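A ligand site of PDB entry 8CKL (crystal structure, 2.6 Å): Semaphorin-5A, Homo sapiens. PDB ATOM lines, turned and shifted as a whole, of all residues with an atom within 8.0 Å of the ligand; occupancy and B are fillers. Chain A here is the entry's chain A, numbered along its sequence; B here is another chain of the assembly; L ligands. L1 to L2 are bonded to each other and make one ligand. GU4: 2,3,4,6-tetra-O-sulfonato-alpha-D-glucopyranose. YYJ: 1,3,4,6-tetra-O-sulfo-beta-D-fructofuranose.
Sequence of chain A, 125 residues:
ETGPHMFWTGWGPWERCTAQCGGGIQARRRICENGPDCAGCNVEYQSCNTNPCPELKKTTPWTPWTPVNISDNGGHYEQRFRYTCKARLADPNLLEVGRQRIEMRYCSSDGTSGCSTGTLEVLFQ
The guanidinium group of Arg 101 of chain B is in salt-bridge range of an oxygen (O25) of GU4 L1. The side-chain carboxylate (OE1) of Glu 55 sits close to an oxygen (O1S3) of YYJ L2 (2.8 Å). The backbone NH (N) of Arg 99 of chain B lies within hydrogen-bond range of an oxygen (O29) of GU4 L1, 2.9 Å away. An oxygen (O24) of GU4 L1 is in salt-bridge range of the guanidinium group (NE) of Arg 99 of chain B (2.9 Å). O28 of GU4 L1 is in hydrogen-bond range of OG1 of Thr 84. The side-chain amino group (NZ) of Lys 86 is in salt-bridge range of an oxygen (O11) of GU4 L1, at 3.2 Å. The side-chain amino group (NZ) of Lys 57 lies within salt-bridge range of an oxygen (O28) of GU4 L1 (3.4 Å).
NZ of Lys 86 is in salt-bridge range of OE2 of Glu 55, 3.9 Å away. The side-chain carboxylate (OE1) of Glu 55 is in salt-bridge range of the guanidinium group (NH2) of Arg 88, at 3.5 Å. The backbone NH (N) of Gly 98 of chain B is in hydrogen-bond range of the backbone carbonyl oxygen (O) of Thr 84, at 2.6 Å. The backbone carbonyl oxygen (O) of Glu 96 of chain B lies within hydrogen-bond range of the backbone NH (N) of Lys 86, at 3.0 Å.
Gly 98 of chain B touches the ligand. Seven residues have an atom within 4 Å of the ligand: Glu 55, Lys 57, Thr 84, Lys 86, Gly 98 of chain B, Arg 99 of chain B and Arg 101 of chain B. The nearest printed residue that does not touch the ligand is Val 97 of chain B (4.8 Å).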
ATOM      1  N   PRO A  54      20.757  -0.833 -11.366  1.00  0.00           N
ATOM      2  CA  PRO A  54      21.280  -0.018 -12.463  1.00  0.00           C
ATOM      3  C   PRO A  54      21.214   1.461 -12.106  1.00  0.00           C
ATOM      4  O   PRO A  54      20.416   1.895 -11.258  1.00  0.00           O
ATOM      5  CB  PRO A  54      20.352  -0.345 -13.642  1.00  0.00           C
ATOM      6  CG  PRO A  54      19.646  -1.605 -13.248  1.00  0.00           C
ATOM      7  CD  PRO A  54      19.532  -1.558 -11.759  1.00  0.00           C
ATOM      8  N   GLU A  55      22.049   2.243 -12.769  1.00  0.00           N
ATOM      9  CA  GLU A  55      22.109   3.684 -12.542  1.00  0.00           C
ATOM     10  C   GLU A  55      21.164   4.369 -13.526  1.00  0.00           C
ATOM     11  O   GLU A  55      21.396   4.340 -14.741  1.00  0.00           O
ATOM     12  CB  GLU A  55      23.538   4.205 -12.676  1.00  0.00           C
ATOM     13  CG  GLU A  55      23.677   5.679 -12.335  1.00  0.00           C
ATOM     14  CD  GLU A  55      25.046   6.004 -11.770  1.00  0.00           C
ATOM     15  OE1 GLU A  55      25.921   5.115 -11.767  1.00  0.00           O
ATOM     16  OE2 GLU A  55      25.230   7.154 -11.306  1.00  0.00           O
ATOM     17  N   LEU A  56      20.121   4.991 -12.994  1.00  0.00           N
ATOM     18  CA  LEU A  56      19.150   5.713 -13.805  1.00  0.00           C
ATOM     19  C   LEU A  56      19.601   7.161 -13.924  1.00  0.00           C
ATOM     20  O   LEU A  56      19.995   7.787 -12.921  1.00  0.00           O
ATOM     21  CB  LEU A  56      17.757   5.649 -13.167  1.00  0.00           C
ATOM     22  CG  LEU A  56      17.314   4.265 -12.686  1.00  0.00           C
ATOM     23  CD1 LEU A  56      15.967   4.350 -12.005  1.00  0.00           C
ATOM     24  CD2 LEU A  56      17.262   3.293 -13.851  1.00  0.00           C
ATOM     25  N   LYS A  57      19.570   7.681 -15.140  1.00  0.00           N
ATOM     26  CA  LYS A  57      20.013   9.036 -15.456  1.00  0.00           C
ATOM     27  C   LYS A  57      18.841   9.781 -16.097  1.00  0.00           C
ATOM     28  O   LYS A  57      18.278   9.315 -17.098  1.00  0.00           O
ATOM     29  CB  LYS A  57      21.222   9.017 -16.391  1.00  0.00           C
ATOM     30  CG  LYS A  57      22.432   8.289 -15.823  1.00  0.00           C
ATOM     31  CD  LYS A  57      23.470   7.944 -16.884  1.00  0.00           C
ATOM     32  CE  LYS A  57      24.248   9.161 -17.361  1.00  0.00           C
ATOM     33  NZ  LYS A  57      23.527   9.989 -18.360  1.00  0.00           N
ATOM     34  N   LYS A  58      18.489  10.927 -15.531  1.00  0.00           N
ATOM     35  CA  LYS A  58      17.426  11.771 -16.067  1.00  0.00           C
ATOM     36  C   LYS A  58      17.962  13.181 -16.258  1.00  0.00           C
ATOM     37  O   LYS A  58      18.498  13.774 -15.324  1.00  0.00           O
ATOM     38  CB  LYS A  58      16.211  11.789 -15.146  1.00  0.00           C
ATOM     39  CG  LYS A  58      15.410  10.493 -15.137  1.00  0.00           C
ATOM     40  CD  LYS A  58      14.060  10.693 -14.470  1.00  0.00           C
ATOM     41  CE  LYS A  58      13.191   9.450 -14.603  1.00  0.00           C
ATOM     42  NZ  LYS A  58      11.836   9.659 -14.009  1.00  0.00           N
ATOM     43  N   THR A  59      17.808  13.722 -17.472  1.00  0.00           N
ATOM     44  CA  THR A  59      18.326  15.042 -17.775  1.00  0.00           C
ATOM     45  C   THR A  59      17.323  16.119 -17.380  1.00  0.00           C
ATOM     46  O   THR A  59      16.107  15.936 -17.521  1.00  0.00           O
ATOM     47  CB  THR A  59      18.696  15.159 -19.253  1.00  0.00           C
ATOM     48  OG1 THR A  59      19.392  16.392 -19.473  1.00  0.00           O
ATOM     49  CG2 THR A  59      17.460  15.118 -20.141  1.00  0.00           C
ATOM     50  N   TYR A  83      21.589  19.762 -16.597  1.00  0.00           N
ATOM     51  CA  TYR A  83      22.234  18.826 -15.691  1.00  0.00           C
ATOM     52  C   TYR A  83      21.557  17.476 -15.775  1.00  0.00           C
ATOM     53  O   TYR A  83      20.503  17.319 -16.401  1.00  0.00           O
ATOM     54  CB  TYR A  83      22.229  19.350 -14.243  1.00  0.00           C
ATOM     55  CG  TYR A  83      23.057  20.593 -14.052  1.00  0.00           C
ATOM     56  CD1 TYR A  83      24.417  20.504 -13.762  1.00  0.00           C
ATOM     57  CD2 TYR A  83      22.496  21.860 -14.140  1.00  0.00           C
ATOM     58  CE1 TYR A  83      25.187  21.635 -13.581  1.00  0.00           C
ATOM     59  CE2 TYR A  83      23.253  22.992 -13.962  1.00  0.00           C
ATOM     60  CZ  TYR A  83      24.599  22.880 -13.683  1.00  0.00           C
ATOM     61  OH  TYR A  83      25.357  24.007 -13.512  1.00  0.00           O
ATOM     62  N   THR A  84      22.178  16.486 -15.150  1.00  0.00           N
ATOM     63  CA  THR A  84      21.657  15.121 -15.121  1.00  0.00           C
ATOM     64  C   THR A  84      21.630  14.614 -13.693  1.00  0.00           C
ATOM     65  O   THR A  84      22.550  14.851 -12.919  1.00  0.00           O
ATOM     66  CB  THR A  84      22.502  14.179 -15.994  1.00  0.00           C
ATOM     67  OG1 THR A  84      23.888  14.315 -15.648  1.00  0.00           O
ATOM     68  CG2 THR A  84      22.315  14.510 -17.469  1.00  0.00           C
ATOM     69  N   CYS A  85      20.550  13.916 -13.352  1.00  0.00           N
ATOM     70  CA  CYS A  85      20.382  13.288 -12.054  1.00  0.00           C
ATOM     71  C   CYS A  85      20.663  11.793 -12.199  1.00  0.00           C
ATOM     72  O   CYS A  85      20.098  11.134 -13.085  1.00  0.00           O
ATOM     73  CB  CYS A  85      18.972  13.500 -11.509  1.00  0.00           C
ATOM     74  SG  CYS A  85      18.411  15.213 -11.438  1.00  0.00           S
ATOM     75  N   LYS A  86      21.538  11.272 -11.343  1.00  0.00           N
ATOM     76  CA  LYS A  86      21.949   9.886 -11.375  1.00  0.00           C
ATOM     77  C   LYS A  86      21.572   9.236 -10.053  1.00  0.00           C
ATOM     78  O   LYS A  86      21.852   9.780  -8.989  1.00  0.00           O
ATOM     79  CB  LYS A  86      23.459   9.765 -11.604  1.00  0.00           C
ATOM     80  CG  LYS A  86      23.953  10.519 -12.824  1.00  0.00           C
ATOM     81  CD  LYS A  86      25.440  10.835 -12.723  1.00  0.00           C
ATOM     82  CE  LYS A  86      26.287   9.577 -12.714  1.00  0.00           C
ATOM     83  NZ  LYS A  86      27.737   9.895 -12.644  1.00  0.00           N
ATOM     84  N   ALA A  87      20.934   8.068 -10.121  1.00  0.00           N
ATOM     85  CA  ALA A  87      20.518   7.383  -8.905  1.00  0.00           C
ATOM     86  C   ALA A  87      20.437   5.884  -9.154  1.00  0.00           C
ATOM     87  O   ALA A  87      19.968   5.455 -10.208  1.00  0.00           O
ATOM     88  CB  ALA A  87      19.170   7.907  -8.406  1.00  0.00           C
ATOM     89  N   ARG A  88      20.891   5.101  -8.178  1.00  0.00           N
ATOM     90  CA  ARG A  88      20.816   3.637  -8.273  1.00  0.00           C
ATOM     91  C   ARG A  88      19.455   3.200  -7.745  1.00  0.00           C
ATOM     92  O   ARG A  88      19.246   3.129  -6.537  1.00  0.00           O
ATOM     93  CB  ARG A  88      21.973   2.995  -7.524  1.00  0.00           C
ATOM     94  CG  ARG A  88      23.327   3.296  -8.137  1.00  0.00           C
ATOM     95  CD  ARG A  88      24.380   2.286  -7.715  1.00  0.00           C
ATOM     96  NE  ARG A  88      25.638   2.492  -8.423  1.00  0.00           N
ATOM     97  CZ  ARG A  88      25.907   2.007  -9.631  1.00  0.00           C
ATOM     98  NH1 ARG A  88      25.026   1.273 -10.286  1.00  0.00           N
ATOM     99  NH2 ARG A  88      27.081   2.272 -10.192  1.00  0.00           N
ATOM    100  N   GLU B  96      23.425  11.331  -6.962  1.00  0.00           N
ATOM    101  CA  GLU B  96      24.489  12.225  -7.396  1.00  0.00           C
ATOM    102  C   GLU B  96      23.985  13.093  -8.549  1.00  0.00           C
ATOM    103  O   GLU B  96      23.050  12.732  -9.265  1.00  0.00           O
ATOM    104  CB  GLU B  96      25.738  11.445  -7.823  1.00  0.00           C
ATOM    105  N   VAL B  97      24.627  14.245  -8.713  1.00  0.00           N
ATOM    106  CA  VAL B  97      24.319  15.182  -9.775  1.00  0.00           C
ATOM    107  C   VAL B  97      25.396  15.071 -10.837  1.00  0.00           C
ATOM    108  O   VAL B  97      26.596  15.060 -10.517  1.00  0.00           O
ATOM    109  CB  VAL B  97      24.208  16.625  -9.254  1.00  0.00           C
ATOM    110  CG1 VAL B  97      23.985  17.598 -10.396  1.00  0.00           C
ATOM    111  CG2 VAL B  97      23.079  16.721  -8.227  1.00  0.00           C
ATOM    112  N   GLY B  98      24.994  14.976 -12.096  1.00  0.00           N
ATOM    113  CA  GLY B  98      25.909  14.733 -13.192  1.00  0.00           C
ATOM    114  C   GLY B  98      26.648  15.965 -13.649  1.00  0.00           C
ATOM    115  O   GLY B  98      26.626  17.039 -13.027  1.00  0.00           O
ATOM    116  N   ARG B  99      27.324  15.815 -14.779  1.00  0.00           N
ATOM    117  CA  ARG B  99      28.144  16.874 -15.343  1.00  0.00           C
ATOM    118  C   ARG B  99      27.270  17.961 -15.966  1.00  0.00           C
ATOM    119  O   ARG B  99      26.116  17.723 -16.350  1.00  0.00           O
ATOM    120  CB  ARG B  99      29.106  16.321 -16.392  1.00  0.00           C
ATOM    121  CG  ARG B  99      28.406  15.691 -17.592  1.00  0.00           C
ATOM    122  CD  ARG B  99      29.389  15.223 -18.641  1.00  0.00           C
ATOM    123  NE  ARG B  99      28.716  14.615 -19.790  1.00  0.00           N
ATOM    124  CZ  ARG B  99      28.334  15.285 -20.870  1.00  0.00           C
ATOM    125  NH1 ARG B  99      28.559  16.577 -21.002  1.00  0.00           N
ATOM    126  NH2 ARG B  99      27.715  14.621 -21.851  1.00  0.00           N
ATOM    127  N   GLN B 100      27.839  19.162 -16.077  1.00  0.00           N
ATOM    128  CA  GLN B 100      27.154  20.279 -16.696  1.00  0.00           C
ATOM    129  C   GLN B 100      27.269  20.179 -18.207  1.00  0.00           C
ATOM    130  O   GLN B 100      28.386  20.131 -18.747  1.00  0.00           O
ATOM    131  CB  GLN B 100      27.734  21.601 -16.193  1.00  0.00           C
ATOM    132  CG  GLN B 100      26.924  22.824 -16.594  1.00  0.00           C
ATOM    133  CD  GLN B 100      27.567  24.126 -16.156  1.00  0.00           C
ATOM    134  OE1 GLN B 100      26.892  25.102 -15.876  1.00  0.00           O
ATOM    135  NE2 GLN B 100      28.897  24.135 -16.103  1.00  0.00           N
ATOM    136  N   ARG B 101      26.129  20.149 -18.896  1.00  0.00           N
ATOM    137  CA  ARG B 101      26.082  20.087 -20.347  1.00  0.00           C
ATOM    138  C   ARG B 101      25.668  21.440 -20.894  1.00  0.00           C
ATOM    139  O   ARG B 101      24.674  22.014 -20.445  1.00  0.00           O
ATOM    140  CB  ARG B 101      25.114  19.002 -20.813  1.00  0.00           C
ATOM    141  CG  ARG B 101      25.487  17.602 -20.364  1.00  0.00           C
ATOM    142  CD  ARG B 101      24.366  16.605 -20.654  1.00  0.00           C
ATOM    143  NE  ARG B 101      24.726  15.252 -20.231  1.00  0.00           N
ATOM    144  CZ  ARG B 101      23.996  14.179 -20.478  1.00  0.00           C
ATOM    145  NH1 ARG B 101      22.858  14.259 -21.138  1.00  0.00           N
ATOM    146  NH2 ARG B 101      24.417  12.989 -20.047  1.00  0.00           N
HETATM  147  C1  GU4 L   1      31.028   9.755 -16.283  1.00  0.00           C
HETATM  148  O5  GU4 L   1      31.593   9.474 -17.620  1.00  0.00           O
HETATM  149  C5  GU4 L   1      30.560   9.294 -18.663  1.00  0.00           C
HETATM  150  C6  GU4 L   1      31.211   9.411 -19.996  1.00  0.00           C
HETATM  151  O6  GU4 L   1      31.860   8.226 -20.332  1.00  0.00           O
HETATM  152  S6  GU4 L   1      32.720   8.300 -21.740  1.00  0.00           S
HETATM  153  O22 GU4 L   1      33.310   6.963 -22.093  1.00  0.00           O
HETATM  154  O23 GU4 L   1      31.803   8.535 -22.915  1.00  0.00           O
HETATM  155  O21 GU4 L   1      33.785   9.364 -21.641  1.00  0.00           O
HETATM  156  C4  GU4 L   1      29.444  10.355 -18.633  1.00  0.00           C
HETATM  157  O4  GU4 L   1      28.329   9.868 -19.392  1.00  0.00           O
HETATM  158  S4  GU4 L   1      27.645  10.946 -20.443  1.00  0.00           S
HETATM  159  O25 GU4 L   1      26.429  11.614 -19.833  1.00  0.00           O
HETATM  160  O26 GU4 L   1      27.029  10.228 -21.625  1.00  0.00           O
HETATM  161  O24 GU4 L   1      28.668  11.964 -20.880  1.00  0.00           O
HETATM  162  C3  GU4 L   1      28.974  10.693 -17.275  1.00  0.00           C
HETATM  163  O3  GU4 L   1      28.159  11.909 -17.413  1.00  0.00           O
HETATM  164  S3  GU4 L   1      26.811  11.963 -16.462  1.00  0.00           S
HETATM  165  O28 GU4 L   1      25.600  12.428 -17.222  1.00  0.00           O
HETATM  166  O29 GU4 L   1      26.969  13.060 -15.446  1.00  0.00           O
HETATM  167  O27 GU4 L   1      26.585  10.627 -15.794  1.00  0.00           O
HETATM  168  C2  GU4 L   1      30.083  10.956 -16.325  1.00  0.00           C
HETATM  169  O2  GU4 L   1      29.556  11.182 -15.015  1.00  0.00           O
HETATM  170  S2  GU4 L   1      30.432  12.184 -14.033  1.00  0.00           S
HETATM  171  O11 GU4 L   1      29.821  12.268 -12.648  1.00  0.00           O
HETATM  172  O12 GU4 L   1      31.793  11.608 -13.716  1.00  0.00           O
HETATM  173  O10 GU4 L   1      30.556  13.553 -14.653  1.00  0.00           O
HETATM  174  C1  YYJ L   2      30.548   7.977 -13.255  1.00  0.00           C
HETATM  175  C2  YYJ L   2      30.754   7.570 -14.689  1.00  0.00           C
HETATM  176  C3  YYJ L   2      29.915   6.349 -15.092  1.00  0.00           C
HETATM  177  C4  YYJ L   2      30.729   5.838 -16.286  1.00  0.00           C
HETATM  178  C5  YYJ L   2      32.162   6.016 -15.800  1.00  0.00           C
HETATM  179  C6  YYJ L   2      33.184   6.263 -16.884  1.00  0.00           C
HETATM  180  O1  YYJ L   2      31.724   8.697 -12.801  1.00  0.00           O
HETATM  181 O1S1 YYJ L   2      33.711   8.943 -11.448  1.00  0.00           O
HETATM  182 O1S3 YYJ L   2      27.659   6.741 -13.287  1.00  0.00           O
HETATM  183 O1S4 YYJ L   2      31.109   4.189 -18.778  1.00  0.00           O
HETATM  184 O1S6 YYJ L   2      36.690   7.433 -16.295  1.00  0.00           O
HETATM  185  O2  YYJ L   2      30.457   8.666 -15.502  1.00  0.00           O
HETATM  186 O2S1 YYJ L   2      33.132   6.827 -12.271  1.00  0.00           O
HETATM  187 O2S3 YYJ L   2      27.158   4.852 -14.845  1.00  0.00           O
HETATM  188 O2S4 YYJ L   2      28.865   4.815 -18.289  1.00  0.00           O
HETATM  189 O2S6 YYJ L   2      35.936   5.716 -18.002  1.00  0.00           O
HETATM  190  O3  YYJ L   2      28.561   6.712 -15.520  1.00  0.00           O
HETATM  191 O3S1 YYJ L   2      31.685   7.698 -10.596  1.00  0.00           O
HETATM  192 O3S3 YYJ L   2      26.211   7.000 -15.165  1.00  0.00           O
HETATM  193 O3S4 YYJ L   2      29.779   2.513 -17.838  1.00  0.00           O
HETATM  194 O3S6 YYJ L   2      35.138   7.957 -17.963  1.00  0.00           O
HETATM  195  O4  YYJ L   2      30.462   4.415 -16.481  1.00  0.00           O
HETATM  196  O5  YYJ L   2      32.116   7.165 -14.933  1.00  0.00           O
HETATM  197  O6  YYJ L   2      34.459   6.472 -16.227  1.00  0.00           O
HETATM  198  S1  YYJ L   2      32.588   8.071 -11.657  1.00  0.00           S
HETATM  199  S3  YYJ L   2      27.369   6.259 -14.594  1.00  0.00           S
HETATM  200  S4  YYJ L   2      29.939   3.942 -17.883  1.00  0.00           S
HETATM  201  S6  YYJ L   2      35.685   6.841 -17.134  1.00  0.00           S
